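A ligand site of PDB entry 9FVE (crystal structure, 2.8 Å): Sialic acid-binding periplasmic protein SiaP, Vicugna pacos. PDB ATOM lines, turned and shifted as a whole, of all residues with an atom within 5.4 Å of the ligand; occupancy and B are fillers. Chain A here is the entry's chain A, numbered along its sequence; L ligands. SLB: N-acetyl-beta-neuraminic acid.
OE2 of Glu 70 lies within hydrogen-bond range of O8 of the ligand (2.5 Å).
OD1 of Asn 189 sits close to O1B of the ligand (2.8 Å).
The guanidinium group of Arg 149 lies within salt-bridge range of an oxygen (O1A) of the ligand (2.8 Å).
O1B of the ligand lies within salt-bridge range of NH2 of Arg 129, 2.8 Å away.
An oxygen (O7) of the ligand is in hydrogen-bond range of the side-chain carboxylate of Asp 52 (3.0 Å).
The side-chain amide nitrogen of Gln 13 lies close to an oxygen (O10) of the ligand (3.4 Å).
The side-chain amide nitrogen (ND2) of Asn 214 sits at hydrogen-bond distance from the side-chain carboxylate (OE1) of Glu 70, at 2.5 Å.
The side-chain amide oxygen (OE1) of Gln 187 is in hydrogen-bond range of the side-chain amide nitrogen (ND2) of Asn 189.
The side-chain carboxylate (OE1) of Glu 188 is in salt-bridge range of the guanidinium group (NE) of Arg 129 (2.7 Å).
The guanidinium group (NE) of Arg 129 lies close to the side-chain amide nitrogen (ND2) of Asn 156 (3.2 Å).
NH1 of Arg 129 lies within hydrogen-bond range of OD1 of Asn 214 (2.7 Å).
The side-chain carboxylate (OD2) of Asp 52 lies within salt-bridge range of the guanidinium group (NH1) of Arg 73.
OH of Tyr 68 lies within hydrogen-bond range of O of Glu 20, 2.4 Å away.
The side-chain sulfur (SD) of Met 85 lies close to the side-chain amide oxygen (OD1) of Asn 156.
Merely in contact with the ligand: Tyr 68 (3.6 Å), Arg 73 (3.7 Å), Met 85 (3.9 Å), Pro 151 (3.6 Å), Phe 172 (3.4 Å) and Gln 216 (3.7 Å).
Hydrophobic or aromatic side chains within 4 Å of the ligand: Tyr 68, Met 85, Pro 151 and Phe 172.
12 residues have an atom within 4 Å of the ligand: Gln 13, Asp 52, Tyr 68, Glu 70, Arg 73, Met 85, Arg 129, Arg 149, Pro 151, Phe 172, Asn 189 and Gln 216.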
ATOM      1  N   GLN A  13      -4.175   4.494   4.045  1.00  0.00           N
ATOM      2  CA  GLN A  13      -5.232   4.839   4.985  1.00  0.00           C
ATOM      3  C   GLN A  13      -6.575   4.244   4.598  1.00  0.00           C
ATOM      4  O   GLN A  13      -7.399   3.953   5.471  1.00  0.00           O
ATOM      5  CB  GLN A  13      -5.371   6.361   5.109  1.00  0.00           C
ATOM      6  CG  GLN A  13      -4.261   7.053   5.869  1.00  0.00           C
ATOM      7  CD  GLN A  13      -4.791   8.177   6.746  1.00  0.00           C
ATOM      8  OE1 GLN A  13      -4.684   8.126   7.969  1.00  0.00           O
ATOM      9  NE2 GLN A  13      -5.379   9.192   6.114  1.00  0.00           N
ATOM     10  N   ALA A  14      -6.834   4.068   3.303  1.00  0.00           N
ATOM     11  CA  ALA A  14      -8.137   3.589   2.858  1.00  0.00           C
ATOM     12  C   ALA A  14      -8.381   2.158   3.316  1.00  0.00           C
ATOM     13  O   ALA A  14      -7.452   1.348   3.436  1.00  0.00           O
ATOM     14  CB  ALA A  14      -8.258   3.679   1.338  1.00  0.00           C
ATOM     15  N   GLU A  20      -9.274   2.743  -3.606  1.00  0.00           N
ATOM     16  CA  GLU A  20      -7.837   2.623  -3.403  1.00  0.00           C
ATOM     17  C   GLU A  20      -7.419   1.213  -3.105  1.00  0.00           C
ATOM     18  O   GLU A  20      -6.359   0.782  -3.566  1.00  0.00           O
ATOM     19  CB  GLU A  20      -7.406   3.521  -2.251  1.00  0.00           C
ATOM     20  CG  GLU A  20      -7.585   5.040  -2.446  1.00  0.00           C
ATOM     21  CD  GLU A  20      -8.920   5.557  -1.889  1.00  0.00           C
ATOM     22  OE1 GLU A  20      -9.933   4.817  -1.937  1.00  0.00           O
ATOM     23  OE2 GLU A  20      -8.977   6.740  -1.471  1.00  0.00           O
ATOM     24  N   ASP A  52      -1.065   8.826   6.372  1.00  0.00           N
ATOM     25  CA  ASP A  52      -0.170   8.987   5.226  1.00  0.00           C
ATOM     26  C   ASP A  52       1.135   9.663   5.625  1.00  0.00           C
ATOM     27  O   ASP A  52       2.208   9.300   5.125  1.00  0.00           O
ATOM     28  CB  ASP A  52      -0.867   9.776   4.121  1.00  0.00           C
ATOM     29  CG  ASP A  52      -1.617  10.984   4.641  1.00  0.00           C
ATOM     30  OD1 ASP A  52      -2.270  11.675   3.831  1.00  0.00           O
ATOM     31  OD2 ASP A  52      -1.559  11.234   5.862  1.00  0.00           O
ATOM     32  N   TYR A  68       0.469   5.429  -0.704  1.00  0.00           N
ATOM     33  CA  TYR A  68      -0.209   6.474  -1.462  1.00  0.00           C
ATOM     34  C   TYR A  68       0.141   7.842  -0.881  1.00  0.00           C
ATOM     35  O   TYR A  68       0.378   7.990   0.319  1.00  0.00           O
ATOM     36  CB  TYR A  68      -1.742   6.359  -1.441  1.00  0.00           C
ATOM     37  CG  TYR A  68      -2.353   5.110  -2.045  1.00  0.00           C
ATOM     38  CD1 TYR A  68      -2.781   5.101  -3.377  1.00  0.00           C
ATOM     39  CD2 TYR A  68      -2.597   3.991  -1.282  1.00  0.00           C
ATOM     40  CE1 TYR A  68      -3.359   3.976  -3.935  1.00  0.00           C
ATOM     41  CE2 TYR A  68      -3.192   2.867  -1.826  1.00  0.00           C
ATOM     42  CZ  TYR A  68      -3.558   2.859  -3.151  1.00  0.00           C
ATOM     43  OH  TYR A  68      -4.134   1.744  -3.701  1.00  0.00           O
ATOM     44  N   ALA A  69       0.156   8.851  -1.750  1.00  0.00           N
ATOM     45  CA  ALA A  69       0.137  10.230  -1.262  1.00  0.00           C
ATOM     46  C   ALA A  69      -0.351  11.151  -2.361  1.00  0.00           C
ATOM     47  O   ALA A  69      -0.115  10.905  -3.546  1.00  0.00           O
ATOM     48  CB  ALA A  69       1.512  10.683  -0.769  1.00  0.00           C
ATOM     49  N   GLU A  70      -1.028  12.220  -1.960  1.00  0.00           N
ATOM     50  CA  GLU A  70      -1.376  13.284  -2.896  1.00  0.00           C
ATOM     51  C   GLU A  70      -0.146  14.131  -3.171  1.00  0.00           C
ATOM     52  O   GLU A  70       0.738  14.286  -2.331  1.00  0.00           O
ATOM     53  CB  GLU A  70      -2.512  14.152  -2.337  1.00  0.00           C
ATOM     54  CG  GLU A  70      -3.670  13.358  -1.743  1.00  0.00           C
ATOM     55  CD  GLU A  70      -4.916  14.201  -1.538  1.00  0.00           C
ATOM     56  OE1 GLU A  70      -5.094  15.200  -2.261  1.00  0.00           O
ATOM     57  OE2 GLU A  70      -5.728  13.851  -0.654  1.00  0.00           O
ATOM     58  N   ARG A  73       0.182  16.806  -0.729  1.00  0.00           N
ATOM     59  CA  ARG A  73       0.606  16.394   0.604  1.00  0.00           C
ATOM     60  C   ARG A  73       2.107  16.522   0.763  1.00  0.00           C
ATOM     61  O   ARG A  73       2.597  16.577   1.903  1.00  0.00           O
ATOM     62  CB  ARG A  73       0.149  14.946   0.843  1.00  0.00           C
ATOM     63  CG  ARG A  73       0.705  14.287   2.093  1.00  0.00           C
ATOM     64  CD  ARG A  73      -0.376  14.098   3.138  1.00  0.00           C
ATOM     65  NE  ARG A  73      -0.719  15.340   3.832  1.00  0.00           N
ATOM     66  CZ  ARG A  73      -1.364  15.382   4.989  1.00  0.00           C
ATOM     67  NH1 ARG A  73      -1.788  14.291   5.585  1.00  0.00           N
ATOM     68  NH2 ARG A  73      -1.582  16.566   5.556  1.00  0.00           N
ATOM     69  N   MET A  85      -2.540  21.772  -4.269  1.00  0.00           N
ATOM     70  CA  MET A  85      -3.768  21.478  -3.553  1.00  0.00           C
ATOM     71  C   MET A  85      -4.582  22.709  -3.134  1.00  0.00           C
ATOM     72  O   MET A  85      -5.672  22.523  -2.590  1.00  0.00           O
ATOM     73  CB  MET A  85      -3.449  20.638  -2.299  1.00  0.00           C
ATOM     74  CG  MET A  85      -4.549  20.623  -1.210  1.00  0.00           C
ATOM     75  SD  MET A  85      -4.435  19.343   0.071  1.00  0.00           S
ATOM     76  CE  MET A  85      -2.659  19.181   0.232  1.00  0.00           C
ATOM     77  N   ARG A 129     -13.203  16.334  -4.010  1.00  0.00           N
ATOM     78  CA  ARG A 129     -13.879  16.255  -2.713  1.00  0.00           C
ATOM     79  C   ARG A 129     -15.148  17.103  -2.709  1.00  0.00           C
ATOM     80  O   ARG A 129     -15.145  18.252  -3.174  1.00  0.00           O
ATOM     81  CB  ARG A 129     -12.950  16.721  -1.599  1.00  0.00           C
ATOM     82  CG  ARG A 129     -11.766  15.823  -1.201  1.00  0.00           C
ATOM     83  CD  ARG A 129     -10.939  16.594  -0.147  1.00  0.00           C
ATOM     84  NE  ARG A 129     -10.788  15.979   1.169  1.00  0.00           N
ATOM     85  CZ  ARG A 129     -10.140  14.847   1.426  1.00  0.00           C
ATOM     86  NH1 ARG A 129      -9.773  14.036   0.449  1.00  0.00           N
ATOM     87  NH2 ARG A 129      -9.856  14.529   2.681  1.00  0.00           N
ATOM     88  N   ARG A 149     -15.517  18.486  10.100  1.00  0.00           N
ATOM     89  CA  ARG A 149     -14.339  17.648  10.239  1.00  0.00           C
ATOM     90  C   ARG A 149     -13.427  17.844   9.025  1.00  0.00           C
ATOM     91  O   ARG A 149     -13.905  17.870   7.886  1.00  0.00           O
ATOM     92  CB  ARG A 149     -14.731  16.171  10.353  1.00  0.00           C
ATOM     93  CG  ARG A 149     -13.549  15.215  10.376  1.00  0.00           C
ATOM     94  CD  ARG A 149     -13.166  14.705   8.993  1.00  0.00           C
ATOM     95  NE  ARG A 149     -11.845  14.080   9.022  1.00  0.00           N
ATOM     96  CZ  ARG A 149     -11.247  13.554   7.962  1.00  0.00           C
ATOM     97  NH1 ARG A 149     -11.798  13.565   6.769  1.00  0.00           N
ATOM     98  NH2 ARG A 149     -10.051  12.989   8.117  1.00  0.00           N
ATOM     99  N   PRO A 151      -9.309  16.518   7.528  1.00  0.00           N
ATOM    100  CA  PRO A 151      -8.061  15.794   7.837  1.00  0.00           C
ATOM    101  C   PRO A 151      -7.027  16.733   8.431  1.00  0.00           C
ATOM    102  O   PRO A 151      -7.177  17.956   8.426  1.00  0.00           O
ATOM    103  CB  PRO A 151      -7.622  15.235   6.476  1.00  0.00           C
ATOM    104  CG  PRO A 151      -8.285  16.122   5.470  1.00  0.00           C
ATOM    105  CD  PRO A 151      -9.609  16.512   6.085  1.00  0.00           C
ATOM    106  N   ALA A 153      -4.702  18.433   7.552  1.00  0.00           N
ATOM    107  CA  ALA A 153      -4.099  19.020   6.357  1.00  0.00           C
ATOM    108  C   ALA A 153      -4.477  20.487   6.282  1.00  0.00           C
ATOM    109  O   ALA A 153      -5.656  20.832   6.396  1.00  0.00           O
ATOM    110  CB  ALA A 153      -4.562  18.285   5.097  1.00  0.00           C
ATOM    111  N   ASN A 156      -7.169  21.641   3.550  1.00  0.00           N
ATOM    112  CA  ASN A 156      -8.520  21.250   3.901  1.00  0.00           C
ATOM    113  C   ASN A 156      -9.056  22.113   5.035  1.00  0.00           C
ATOM    114  O   ASN A 156     -10.248  22.460   5.049  1.00  0.00           O
ATOM    115  CB  ASN A 156      -8.563  19.775   4.296  1.00  0.00           C
ATOM    116  CG  ASN A 156      -8.046  18.856   3.212  1.00  0.00           C
ATOM    117  OD1 ASN A 156      -6.845  18.811   2.948  1.00  0.00           O
ATOM    118  ND2 ASN A 156      -8.949  18.142   2.551  1.00  0.00           N
ATOM    119  N   PHE A 172      -9.120   9.904   9.760  1.00  0.00           N
ATOM    120  CA  PHE A 172     -10.097   9.369   8.805  1.00  0.00           C
ATOM    121  C   PHE A 172     -10.879   8.206   9.404  1.00  0.00           C
ATOM    122  O   PHE A 172     -12.038   7.985   9.042  1.00  0.00           O
ATOM    123  CB  PHE A 172      -9.352   8.967   7.519  1.00  0.00           C
ATOM    124  CG  PHE A 172     -10.247   8.599   6.369  1.00  0.00           C
ATOM    125  CD1 PHE A 172     -11.260   9.438   5.957  1.00  0.00           C
ATOM    126  CD2 PHE A 172     -10.040   7.426   5.659  1.00  0.00           C
ATOM    127  CE1 PHE A 172     -12.075   9.106   4.890  1.00  0.00           C
ATOM    128  CE2 PHE A 172     -10.842   7.084   4.600  1.00  0.00           C
ATOM    129  CZ  PHE A 172     -11.871   7.924   4.212  1.00  0.00           C
ATOM    130  N   GLN A 187     -18.369  16.814   6.986  1.00  0.00           N
ATOM    131  CA  GLN A 187     -17.098  16.340   6.461  1.00  0.00           C
ATOM    132  C   GLN A 187     -17.062  16.540   4.949  1.00  0.00           C
ATOM    133  O   GLN A 187     -18.071  16.851   4.308  1.00  0.00           O
ATOM    134  CB  GLN A 187     -16.857  14.884   6.843  1.00  0.00           C
ATOM    135  CG  GLN A 187     -17.712  13.864   6.092  1.00  0.00           C
ATOM    136  CD  GLN A 187     -17.102  13.478   4.752  1.00  0.00           C
ATOM    137  OE1 GLN A 187     -15.916  13.145   4.667  1.00  0.00           O
ATOM    138  NE2 GLN A 187     -17.919  13.498   3.700  1.00  0.00           N
ATOM    139  N   GLU A 188     -15.872  16.332   4.370  1.00  0.00           N
ATOM    140  CA  GLU A 188     -15.608  16.592   2.957  1.00  0.00           C
ATOM    141  C   GLU A 188     -14.658  15.542   2.402  1.00  0.00           C
ATOM    142  O   GLU A 188     -13.592  15.307   2.973  1.00  0.00           O
ATOM    143  CB  GLU A 188     -15.037  18.004   2.777  1.00  0.00           C
ATOM    144  CG  GLU A 188     -13.857  18.346   3.691  1.00  0.00           C
ATOM    145  CD  GLU A 188     -12.504  18.075   3.060  1.00  0.00           C
ATOM    146  OE1 GLU A 188     -12.423  18.005   1.815  1.00  0.00           O
ATOM    147  OE2 GLU A 188     -11.511  17.953   3.804  1.00  0.00           O
ATOM    148  N   ASN A 189     -15.036  14.918   1.289  1.00  0.00           N
ATOM    149  CA  ASN A 189     -14.268  13.809   0.748  1.00  0.00           C
ATOM    150  C   ASN A 189     -14.685  13.581  -0.704  1.00  0.00           C
ATOM    151  O   ASN A 189     -15.634  14.214  -1.186  1.00  0.00           O
ATOM    152  CB  ASN A 189     -14.490  12.534   1.569  1.00  0.00           C
ATOM    153  CG  ASN A 189     -13.346  12.235   2.497  1.00  0.00           C
ATOM    154  OD1 ASN A 189     -12.229  11.957   2.053  1.00  0.00           O
ATOM    155  ND2 ASN A 189     -13.610  12.289   3.795  1.00  0.00           N
ATOM    156  N   ASN A 214      -8.124  15.560  -5.824  1.00  0.00           N
ATOM    157  CA  ASN A 214      -7.149  14.676  -5.215  1.00  0.00           C
ATOM    158  C   ASN A 214      -6.522  13.837  -6.310  1.00  0.00           C
ATOM    159  O   ASN A 214      -7.215  13.072  -6.993  1.00  0.00           O
ATOM    160  CB  ASN A 214      -7.793  13.789  -4.144  1.00  0.00           C
ATOM    161  CG  ASN A 214      -8.226  14.559  -2.903  1.00  0.00           C
ATOM    162  OD1 ASN A 214      -9.125  14.147  -2.179  1.00  0.00           O
ATOM    163  ND2 ASN A 214      -7.562  15.683  -2.650  1.00  0.00           N
ATOM    164  N   GLN A 216      -3.356  10.850  -6.466  1.00  0.00           N
ATOM    165  CA  GLN A 216      -2.918   9.883  -5.455  1.00  0.00           C
ATOM    166  C   GLN A 216      -1.638   9.265  -6.023  1.00  0.00           C
ATOM    167  O   GLN A 216      -1.689   8.315  -6.805  1.00  0.00           O
ATOM    168  CB  GLN A 216      -4.005   8.853  -5.219  1.00  0.00           C
ATOM    169  CG  GLN A 216      -3.903   7.808  -4.148  1.00  0.00           C
ATOM    170  CD  GLN A 216      -4.524   8.270  -2.863  1.00  0.00           C
ATOM    171  OE1 GLN A 216      -4.764   9.466  -2.671  1.00  0.00           O
ATOM    172  NE2 GLN A 216      -4.957   7.326  -2.039  1.00  0.00           N
HETATM  173  C1  SLB L   1      -9.622  12.036   4.518  1.00  0.00           C
HETATM  174  C2  SLB L   1      -8.819  11.561   3.316  1.00  0.00           C
HETATM  175  C3  SLB L   1      -8.611  10.045   3.412  1.00  0.00           C
HETATM  176  C4  SLB L   1      -7.575   9.583   2.383  1.00  0.00           C
HETATM  177  C5  SLB L   1      -6.291  10.385   2.583  1.00  0.00           C
HETATM  178  C6  SLB L   1      -6.603  11.880   2.480  1.00  0.00           C
HETATM  179  C7  SLB L   1      -5.339  12.635   2.872  1.00  0.00           C
HETATM  180  C8  SLB L   1      -5.393  14.142   2.640  1.00  0.00           C
HETATM  181  C9  SLB L   1      -3.983  14.516   2.185  1.00  0.00           C
HETATM  182  C10 SLB L   1      -4.210   9.122   1.925  1.00  0.00           C
HETATM  183  C11 SLB L   1      -3.192   8.707   0.855  1.00  0.00           C
HETATM  184  N5  SLB L   1      -5.324   9.983   1.565  1.00  0.00           N
HETATM  185  O1A SLB L   1      -9.113  12.021   5.658  1.00  0.00           O
HETATM  186  O1B SLB L   1     -10.790  12.481   4.355  1.00  0.00           O
HETATM  187  O4  SLB L   1      -7.307   8.223   2.557  1.00  0.00           O
HETATM  188  O6  SLB L   1      -7.597  12.233   3.384  1.00  0.00           O
HETATM  189  O7  SLB L   1      -5.119  12.396   4.248  1.00  0.00           O
HETATM  190  O8  SLB L   1      -6.333  14.449   1.666  1.00  0.00           O
HETATM  191  O9  SLB L   1      -3.891  15.868   1.880  1.00  0.00           O
HETATM  192  O10 SLB L   1      -4.069   8.752   3.040  1.00  0.00           O
